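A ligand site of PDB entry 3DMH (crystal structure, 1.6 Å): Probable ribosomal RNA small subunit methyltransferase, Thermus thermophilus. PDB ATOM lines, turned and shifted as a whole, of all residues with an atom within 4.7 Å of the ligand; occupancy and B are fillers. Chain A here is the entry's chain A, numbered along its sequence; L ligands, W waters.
Residues that only touch the ligand: Phe 207 (3.4 Å), Gly 243 (3.5 Å), Ala 246 (3.5 Å), Leu 247 (3.99 Å), Ser 287 (3.6 Å), Pro 306 (3.4 Å), Pro 307 (3.7 Å), Val 318 (3.6 Å) and Phe 322 (3.8 Å).
Hydrophobic or aromatic side chains within 4 Å of the ligand: Phe 207, Ala 246, Leu 247, Val 289, Pro 307, Val 318 and Phe 322.
Of the 24 residues printed, 18 come within 4 Å of the ligand.
The nearest printed residue that does not touch the ligand is Asp 264 (4.1 Å).
The backbone NH (N) of Ser 287 is in hydrogen-bond range of the backbone carbonyl oxygen (O) of Glu 262, 2.9 Å away.
N of Asp 264 is in hydrogen-bond range of OE2 of Glu 262, 3.0 Å away.
N of Ala 242 lies within hydrogen-bond range of O of Val 261 (3.0 Å).
The side-chain hydroxyl (OG) of Ser 216 lies within hydrogen-bond range of the side-chain amide nitrogen (ND2) of Asn 305.
The side-chain hydroxyl (OH) of Tyr 8 is in hydrogen-bond range of the side-chain carboxylate (OD1) of Asp 288 (2.6 Å).
The backbone NH of Gly 241 is in hydrogen-bond range of the backbone carbonyl oxygen of Val 261 (2.8 Å).
The backbone NH of Gly 243 is in hydrogen-bond range of the side-chain carboxylate of Glu 262 (2.8 Å).
The backbone NH (N) of Asp 263 sits close to the backbone carbonyl oxygen (O) of Ser 287 (3.2 Å).
N1 of the ligand sits at hydrogen-bond distance from O of Gly 241 (2.8 Å).
N of Asp 263 sits at hydrogen-bond distance from N6 of the ligand (3.3 Å).
An oxygen (O5) of the ligand sits at hydrogen-bond distance from the side-chain carboxylate (OE2) of Glu 262, at 2.6 Å.
The side-chain hydroxyl of Tyr 8 is in hydrogen-bond range of a nitrogen (N4) of the ligand, 3.3 Å away.
The backbone carbonyl oxygen (O) of Ala 242 lies close to a nitrogen (N1) of the ligand (3.4 Å).
An oxygen (O1) of the ligand is in hydrogen-bond range of the side-chain amide nitrogen of Asn 305 (3.5 Å).
N4 of the ligand lies within hydrogen-bond range of OD1 of Asp 288, at 2.9 Å.
N of Val 289 is in hydrogen-bond range of N5 of the ligand (2.9 Å).
The side-chain hydroxyl of Ser 216 lies within hydrogen-bond range of an oxygen (O1) of the ligand, at 2.6 Å.
Water W1 lies within hydrogen-bond range of the side-chain hydroxyl (OG) of Ser 267 (2.7 Å), an oxygen (O4) of the ligand (2.7 Å) and the backbone NH (N) of Phe 207 (2.9 Å).
Water W8 lies within hydrogen-bond range of an oxygen (O2) of the ligand (2.8 Å) and the backbone NH (N) of Asp 213 (2.9 Å).
Water W9 lies within hydrogen-bond range of O2 of the ligand (2.8 Å) and N of Ala 246 (3.0 Å).
Water W11 lies within hydrogen-bond range of the side-chain carboxylate (OD1) of Asp 239 (2.7 Å), a nitrogen (N1) of the ligand (2.9 Å), the backbone NH (N) of Asn 305 (3.0 Å) and the backbone carbonyl oxygen (O) of Gly 241 (3.1 Å).
Water W3 lies within hydrogen-bond range of the side-chain carboxylate (OD2) of Asp 239 (2.6 Å), the backbone carbonyl oxygen (O) of Ala 242 (2.6 Å), a nitrogen (N1) of the ligand (2.9 Å) and the backbone NH (N) of Leu 247 (3.0 Å).
Water W6 bridges OD2 of Asp 263 (3.0 Å) and N4 of the ligand (3.0 Å).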
ATOM      1  N   TYR A   8      37.204 -15.446   5.793  1.00  0.00           N
ATOM      2  CA  TYR A   8      36.121 -15.572   4.835  1.00  0.00           C
ATOM      3  C   TYR A   8      35.910 -17.041   4.399  1.00  0.00           C
ATOM      4  O   TYR A   8      34.760 -17.490   4.281  1.00  0.00           O
ATOM      5  CB  TYR A   8      36.315 -14.663   3.579  1.00  0.00           C
ATOM      6  CG  TYR A   8      35.164 -14.968   2.633  1.00  0.00           C
ATOM      7  CD1 TYR A   8      33.903 -14.418   2.861  1.00  0.00           C
ATOM      8  CD2 TYR A   8      35.282 -15.925   1.601  1.00  0.00           C
ATOM      9  CE1 TYR A   8      32.804 -14.742   2.107  1.00  0.00           C
ATOM     10  CE2 TYR A   8      34.186 -16.267   0.820  1.00  0.00           C
ATOM     11  CZ  TYR A   8      32.937 -15.685   1.061  1.00  0.00           C
ATOM     12  OH  TYR A   8      31.842 -16.058   0.337  1.00  0.00           O
ATOM     13  N   PHE A 207      21.344 -12.378 -11.364  1.00  0.00           N
ATOM     14  CA  PHE A 207      21.318 -10.923 -11.177  1.00  0.00           C
ATOM     15  C   PHE A 207      21.060 -10.235 -12.516  1.00  0.00           C
ATOM     16  O   PHE A 207      21.681 -10.579 -13.538  1.00  0.00           O
ATOM     17  CB  PHE A 207      22.655 -10.438 -10.614  1.00  0.00           C
ATOM     18  CG  PHE A 207      22.757  -8.947 -10.530  1.00  0.00           C
ATOM     19  CD1 PHE A 207      22.096  -8.261  -9.520  1.00  0.00           C
ATOM     20  CD2 PHE A 207      23.524  -8.217 -11.451  1.00  0.00           C
ATOM     21  CE1 PHE A 207      22.172  -6.867  -9.425  1.00  0.00           C
ATOM     22  CE2 PHE A 207      23.618  -6.831 -11.366  1.00  0.00           C
ATOM     23  CZ  PHE A 207      22.941  -6.159 -10.342  1.00  0.00           C
ATOM     24  N   ASP A 213      22.962  -4.532 -16.374  1.00  0.00           N
ATOM     25  CA  ASP A 213      22.995  -3.579 -15.254  1.00  0.00           C
ATOM     26  C   ASP A 213      23.711  -2.290 -15.697  1.00  0.00           C
ATOM     27  O   ASP A 213      24.844  -2.345 -16.163  1.00  0.00           O
ATOM     28  CB  ASP A 213      23.734  -4.229 -14.055  1.00  0.00           C
ATOM     29  CG  ASP A 213      23.792  -3.333 -12.814  1.00  0.00           C
ATOM     30  OD1 ASP A 213      23.387  -2.150 -12.852  1.00  0.00           O
ATOM     31  OD2 ASP A 213      24.267  -3.821 -11.763  1.00  0.00           O
ATOM     32  N   SER A 216      27.242  -2.084 -14.488  1.00  0.00           N
ATOM     33  CA  SER A 216      28.218  -2.862 -15.256  1.00  0.00           C
ATOM     34  C   SER A 216      28.669  -2.093 -16.510  1.00  0.00           C
ATOM     35  O   SER A 216      29.866  -2.049 -16.829  1.00  0.00           O
ATOM     36  CB  SER A 216      27.605  -4.212 -15.642  1.00  0.00           C
ATOM     37  OG  SER A 216      27.172  -4.925 -14.492  1.00  0.00           O
ATOM     38  N   ASP A 239      37.097 -11.805 -13.176  1.00  0.00           N
ATOM     39  CA  ASP A 239      35.802 -11.144 -12.997  1.00  0.00           C
ATOM     40  C   ASP A 239      35.199 -11.754 -11.727  1.00  0.00           C
ATOM     41  O   ASP A 239      34.787 -12.939 -11.747  1.00  0.00           O
ATOM     42  CB  ASP A 239      34.915 -11.384 -14.220  1.00  0.00           C
ATOM     43  CG  ASP A 239      33.551 -10.700 -14.141  1.00  0.00           C
ATOM     44  OD1 ASP A 239      33.194 -10.143 -13.097  1.00  0.00           O
ATOM     45  OD2 ASP A 239      32.840 -10.772 -15.159  1.00  0.00           O
ATOM     46  N   GLY A 241      32.459 -12.486  -9.328  1.00  0.00           N
ATOM     47  CA  GLY A 241      31.011 -12.491  -9.340  1.00  0.00           C
ATOM     48  C   GLY A 241      30.541 -12.268 -10.759  1.00  0.00           C
ATOM     49  O   GLY A 241      29.851 -11.309 -11.041  1.00  0.00           O
ATOM     50  N   ALA A 242      30.916 -13.179 -11.653  1.00  0.00           N
ATOM     51  CA  ALA A 242      30.770 -12.921 -13.103  1.00  0.00           C
ATOM     52  C   ALA A 242      29.320 -12.921 -13.607  1.00  0.00           C
ATOM     53  O   ALA A 242      29.041 -12.337 -14.677  1.00  0.00           O
ATOM     54  CB  ALA A 242      31.631 -13.937 -13.945  1.00  0.00           C
ATOM     55  N   GLY A 243      28.397 -13.539 -12.876  1.00  0.00           N
ATOM     56  CA  GLY A 243      27.012 -13.598 -13.335  1.00  0.00           C
ATOM     57  C   GLY A 243      26.875 -14.244 -14.709  1.00  0.00           C
ATOM     58  O   GLY A 243      27.645 -15.146 -15.031  1.00  0.00           O
ATOM     59  N   ALA A 246      27.976  -9.995 -18.073  1.00  0.00           N
ATOM     60  CA  ALA A 246      27.924  -8.586 -18.540  1.00  0.00           C
ATOM     61  C   ALA A 246      29.309  -7.953 -18.657  1.00  0.00           C
ATOM     62  O   ALA A 246      29.555  -7.184 -19.593  1.00  0.00           O
ATOM     63  CB  ALA A 246      27.020  -7.740 -17.650  1.00  0.00           C
ATOM     64  N   LEU A 247      30.220  -8.274 -17.735  1.00  0.00           N
ATOM     65  CA  LEU A 247      31.623  -7.820 -17.839  1.00  0.00           C
ATOM     66  C   LEU A 247      32.491  -8.822 -18.613  1.00  0.00           C
ATOM     67  O   LEU A 247      33.376  -8.439 -19.375  1.00  0.00           O
ATOM     68  CB  LEU A 247      32.240  -7.571 -16.457  1.00  0.00           C
ATOM     69  CG  LEU A 247      31.472  -6.624 -15.528  1.00  0.00           C
ATOM     70  CD1 LEU A 247      32.163  -6.489 -14.183  1.00  0.00           C
ATOM     71  CD2 LEU A 247      31.288  -5.239 -16.162  1.00  0.00           C
ATOM     72  N   VAL A 261      34.636 -15.985 -11.816  1.00  0.00           N
ATOM     73  CA  VAL A 261      34.274 -16.796 -10.644  1.00  0.00           C
ATOM     74  C   VAL A 261      32.892 -16.380 -10.202  1.00  0.00           C
ATOM     75  O   VAL A 261      32.555 -15.194 -10.166  1.00  0.00           O
ATOM     76  CB  VAL A 261      35.276 -16.700  -9.476  1.00  0.00           C
ATOM     77  CG1 VAL A 261      36.595 -17.395  -9.856  1.00  0.00           C
ATOM     78  CG2 VAL A 261      35.573 -15.263  -8.992  1.00  0.00           C
ATOM     79  N   GLU A 262      32.069 -17.377  -9.899  1.00  0.00           N
ATOM     80  CA  GLU A 262      30.647 -17.140  -9.633  1.00  0.00           C
ATOM     81  C   GLU A 262      30.145 -18.240  -8.697  1.00  0.00           C
ATOM     82  O   GLU A 262      30.372 -19.444  -8.984  1.00  0.00           O
ATOM     83  CB  GLU A 262      29.891 -17.140 -10.968  1.00  0.00           C
ATOM     84  CG  GLU A 262      28.377 -17.157 -10.857  1.00  0.00           C
ATOM     85  CD  GLU A 262      27.837 -16.001 -10.025  1.00  0.00           C
ATOM     86  OE1 GLU A 262      28.088 -14.840 -10.404  1.00  0.00           O
ATOM     87  OE2 GLU A 262      27.170 -16.278  -9.019  1.00  0.00           O
ATOM     88  N   ASP A 263      29.512 -17.880  -7.585  1.00  0.00           N
ATOM     89  CA  ASP A 263      29.111 -18.862  -6.590  1.00  0.00           C
ATOM     90  C   ASP A 263      27.840 -19.605  -6.987  1.00  0.00           C
ATOM     91  O   ASP A 263      27.583 -20.681  -6.440  1.00  0.00           O
ATOM     92  CB  ASP A 263      28.879 -18.143  -5.263  1.00  0.00           C
ATOM     93  CG  ASP A 263      28.613 -19.092  -4.105  1.00  0.00           C
ATOM     94  OD1 ASP A 263      29.522 -19.877  -3.758  1.00  0.00           O
ATOM     95  OD2 ASP A 263      27.494 -19.010  -3.502  1.00  0.00           O
ATOM     96  N   ASP A 264      27.024 -18.987  -7.843  1.00  0.00           N
ATOM     97  CA  ASP A 264      25.725 -19.555  -8.190  1.00  0.00           C
ATOM     98  C   ASP A 264      25.775 -20.392  -9.474  1.00  0.00           C
ATOM     99  O   ASP A 264      26.111 -19.881 -10.522  1.00  0.00           O
ATOM    100  CB  ASP A 264      24.675 -18.424  -8.365  1.00  0.00           C
ATOM    101  CG  ASP A 264      23.416 -18.923  -9.005  1.00  0.00           C
ATOM    102  OD1 ASP A 264      22.915 -19.955  -8.565  1.00  0.00           O
ATOM    103  OD2 ASP A 264      22.931 -18.270  -9.975  1.00  0.00           O
ATOM    104  N   SER A 267      23.995 -19.152 -12.607  1.00  0.00           N
ATOM    105  CA  SER A 267      24.737 -18.091 -13.233  1.00  0.00           C
ATOM    106  C   SER A 267      25.954 -18.601 -14.007  1.00  0.00           C
ATOM    107  O   SER A 267      26.230 -18.135 -15.112  1.00  0.00           O
ATOM    108  CB  SER A 267      25.166 -17.051 -12.182  1.00  0.00           C
ATOM    109  OG  SER A 267      24.015 -16.371 -11.694  1.00  0.00           O
ATOM    110  N   SER A 287      32.593 -21.121  -8.147  1.00  0.00           N
ATOM    111  CA  SER A 287      33.594 -20.850  -7.127  1.00  0.00           C
ATOM    112  C   SER A 287      33.026 -19.896  -6.078  1.00  0.00           C
ATOM    113  O   SER A 287      32.320 -18.944  -6.418  1.00  0.00           O
ATOM    114  CB  SER A 287      34.763 -20.124  -7.793  1.00  0.00           C
ATOM    115  OG  SER A 287      35.851 -19.951  -6.906  1.00  0.00           O
ATOM    116  N   ASP A 288      33.370 -20.154  -4.823  1.00  0.00           N
ATOM    117  CA  ASP A 288      33.082 -19.228  -3.726  1.00  0.00           C
ATOM    118  C   ASP A 288      34.259 -18.253  -3.704  1.00  0.00           C
ATOM    119  O   ASP A 288      35.355 -18.611  -3.286  1.00  0.00           O
ATOM    120  CB  ASP A 288      32.977 -19.992  -2.406  1.00  0.00           C
ATOM    121  CG  ASP A 288      32.717 -19.084  -1.206  1.00  0.00           C
ATOM    122  OD1 ASP A 288      32.359 -17.904  -1.412  1.00  0.00           O
ATOM    123  OD2 ASP A 288      32.851 -19.574  -0.057  1.00  0.00           O
ATOM    124  N   VAL A 289      34.040 -17.050  -4.236  1.00  0.00           N
ATOM    125  CA  VAL A 289      35.100 -16.055  -4.452  1.00  0.00           C
ATOM    126  C   VAL A 289      36.242 -16.765  -5.220  1.00  0.00           C
ATOM    127  O   VAL A 289      35.991 -17.311  -6.305  1.00  0.00           O
ATOM    128  CB  VAL A 289      35.555 -15.303  -3.142  1.00  0.00           C
ATOM    129  CG1 VAL A 289      36.317 -14.041  -3.491  1.00  0.00           C
ATOM    130  CG2 VAL A 289      34.327 -14.878  -2.329  1.00  0.00           C
ATOM    131  N   ASN A 305      31.431  -6.051 -10.083  1.00  0.00           N
ATOM    132  CA  ASN A 305      30.193  -5.400  -9.673  1.00  0.00           C
ATOM    133  C   ASN A 305      29.685  -6.281  -8.513  1.00  0.00           C
ATOM    134  O   ASN A 305      28.997  -7.275  -8.767  1.00  0.00           O
ATOM    135  CB  ASN A 305      29.224  -5.406 -10.862  1.00  0.00           C
ATOM    136  CG  ASN A 305      27.886  -4.784 -10.547  1.00  0.00           C
ATOM    137  OD1 ASN A 305      27.646  -4.321  -9.435  1.00  0.00           O
ATOM    138  ND2 ASN A 305      26.988  -4.759 -11.545  1.00  0.00           N
ATOM    139  N   PRO A 306      30.095  -5.977  -7.274  1.00  0.00           N
ATOM    140  CA  PRO A 306      29.821  -6.942  -6.193  1.00  0.00           C
ATOM    141  C   PRO A 306      28.359  -7.067  -5.811  1.00  0.00           C
ATOM    142  O   PRO A 306      27.544  -6.155  -6.070  1.00  0.00           O
ATOM    143  CB  PRO A 306      30.601  -6.392  -4.990  1.00  0.00           C
ATOM    144  CG  PRO A 306      31.420  -5.281  -5.470  1.00  0.00           C
ATOM    145  CD  PRO A 306      30.867  -4.808  -6.797  1.00  0.00           C
ATOM    146  N   PRO A 307      28.014  -8.161  -5.108  1.00  0.00           N
ATOM    147  CA  PRO A 307      26.667  -8.278  -4.554  1.00  0.00           C
ATOM    148  C   PRO A 307      26.415  -7.198  -3.491  1.00  0.00           C
ATOM    149  O   PRO A 307      27.368  -6.684  -2.903  1.00  0.00           O
ATOM    150  CB  PRO A 307      26.658  -9.665  -3.910  1.00  0.00           C
ATOM    151  CG  PRO A 307      28.105  -9.963  -3.654  1.00  0.00           C
ATOM    152  CD  PRO A 307      28.895  -9.274  -4.713  1.00  0.00           C
ATOM    153  N   PHE A 308      25.146  -6.894  -3.254  1.00  0.00           N
ATOM    154  CA  PHE A 308      24.814  -5.845  -2.310  1.00  0.00           C
ATOM    155  C   PHE A 308      23.496  -6.177  -1.646  1.00  0.00           C
ATOM    156  O   PHE A 308      22.682  -6.920  -2.192  1.00  0.00           O
ATOM    157  CB  PHE A 308      24.770  -4.483  -3.005  1.00  0.00           C
ATOM    158  CG  PHE A 308      23.834  -4.431  -4.178  1.00  0.00           C
ATOM    159  CD1 PHE A 308      22.526  -3.970  -4.030  1.00  0.00           C
ATOM    160  CD2 PHE A 308      24.263  -4.838  -5.444  1.00  0.00           C
ATOM    161  CE1 PHE A 308      21.666  -3.926  -5.117  1.00  0.00           C
ATOM    162  CE2 PHE A 308      23.399  -4.803  -6.529  1.00  0.00           C
ATOM    163  CZ  PHE A 308      22.107  -4.356  -6.369  1.00  0.00           C
ATOM    164  N   VAL A 318      30.744 -11.009   1.472  1.00  0.00           N
ATOM    165  CA  VAL A 318      31.273 -11.461   0.174  1.00  0.00           C
ATOM    166  C   VAL A 318      31.949 -10.312  -0.554  1.00  0.00           C
ATOM    167  O   VAL A 318      33.049 -10.475  -1.109  1.00  0.00           O
ATOM    168  CB  VAL A 318      30.183 -12.085  -0.726  1.00  0.00           C
ATOM    169  CG1 VAL A 318      30.694 -12.322  -2.157  1.00  0.00           C
ATOM    170  CG2 VAL A 318      29.648 -13.389  -0.105  1.00  0.00           C
ATOM    171  N   PHE A 322      35.752  -9.768  -1.828  1.00  0.00           N
ATOM    172  CA  PHE A 322      36.117  -9.466  -3.207  1.00  0.00           C
ATOM    173  C   PHE A 322      37.278  -8.474  -3.227  1.00  0.00           C
ATOM    174  O   PHE A 322      38.229  -8.649  -3.979  1.00  0.00           O
ATOM    175  CB  PHE A 322      34.931  -8.870  -3.959  1.00  0.00           C
ATOM    176  CG  PHE A 322      33.970  -9.881  -4.530  1.00  0.00           C
ATOM    177  CD1 PHE A 322      33.987 -11.236  -4.171  1.00  0.00           C
ATOM    178  CD2 PHE A 322      32.996  -9.447  -5.446  1.00  0.00           C
ATOM    179  CE1 PHE A 322      33.076 -12.115  -4.753  1.00  0.00           C
ATOM    180  CE2 PHE A 322      32.091 -10.313  -6.010  1.00  0.00           C
ATOM    181  CZ  PHE A 322      32.132 -11.659  -5.666  1.00  0.00           C
HETATM  182  N1  LIG L   1      29.204  -9.381 -12.984  1.00  0.00           N
HETATM  183  C1  LIG L   1      27.735  -9.535 -13.240  1.00  0.00           C
HETATM  184  C2  LIG L   1      27.202  -8.251 -13.838  1.00  0.00           C
HETATM  185  O1  LIG L   1      27.956  -7.269 -13.763  1.00  0.00           O
HETATM  186  O2  LIG L   1      26.056  -8.216 -14.309  1.00  0.00           O
HETATM  187  C3  LIG L   1      26.970  -9.840 -11.952  1.00  0.00           C
HETATM  188  C4  LIG L   1      27.077  -8.776 -10.852  1.00  0.00           C
HETATM  189  S1  LIG L   1      26.027  -9.191  -9.420  1.00  0.00           S
HETATM  190  C5  LIG L   1      25.817  -7.560  -8.645  1.00  0.00           C
HETATM  191  C6  LIG L   1      27.132  -9.977  -8.212  1.00  0.00           C
HETATM  192  C7  LIG L   1      27.433 -11.431  -8.560  1.00  0.00           C
HETATM  193  O3  LIG L   1      28.207 -11.925  -7.478  1.00  0.00           O
HETATM  194  C8  LIG L   1      26.196 -12.327  -8.715  1.00  0.00           C
HETATM  195  O4  LIG L   1      26.190 -13.004  -9.964  1.00  0.00           O
HETATM  196  C9  LIG L   1      26.315 -13.282  -7.524  1.00  0.00           C
HETATM  197  O5  LIG L   1      25.751 -14.572  -7.722  1.00  0.00           O
HETATM  198  C10 LIG L   1      27.833 -13.275  -7.346  1.00  0.00           C
HETATM  199  N2  LIG L   1      28.228 -13.796  -6.055  1.00  0.00           N
HETATM  200  C11 LIG L   1      27.552 -13.724  -4.840  1.00  0.00           C
HETATM  201  N3  LIG L   1      28.306 -14.316  -3.880  1.00  0.00           N
HETATM  202  C12 LIG L   1      29.456 -14.792  -4.480  1.00  0.00           C
HETATM  203  C13 LIG L   1      30.554 -15.512  -4.022  1.00  0.00           C
HETATM  204  N4  LIG L   1      30.651 -15.914  -2.744  1.00  0.00           N
HETATM  205  N5  LIG L   1      31.547 -15.816  -4.927  1.00  0.00           N
HETATM  206  C14 LIG L   1      31.456 -15.450  -6.250  1.00  0.00           C
HETATM  207  N6  LIG L   1      30.349 -14.779  -6.748  1.00  0.00           N
HETATM  208  C15 LIG L   1      29.385 -14.456  -5.851  1.00  0.00           C
HETATM  209  O   HOH W   1      23.956 -13.667 -11.413  1.00  0.00           O
HETATM  210  O   HOH W   2      24.591 -15.897  -5.454  1.00  0.00           O
HETATM  211  O   HOH W   3      30.373 -10.223 -15.511  1.00  0.00           O
HETATM  212  O   HOH W   4      24.103 -10.359  -6.784  1.00  0.00           O
HETATM  213  O   HOH W   5      24.534 -12.486  -4.452  1.00  0.00           O
HETATM  214  O   HOH W   6      27.976 -16.804  -1.601  1.00  0.00           O
HETATM  215  O   HOH W   7      26.348 -14.445  -1.713  1.00  0.00           O
HETATM  216  O   HOH W   8      24.145  -7.120 -15.996  1.00  0.00           O
HETATM  217  O   HOH W   9      25.996 -10.542 -15.954  1.00  0.00           O
HETATM  218  O   HOH W  10      22.738 -14.449  -8.333  1.00  0.00           O
HETATM  219  O   HOH W  11      31.530  -8.769 -11.421  1.00  0.00           O
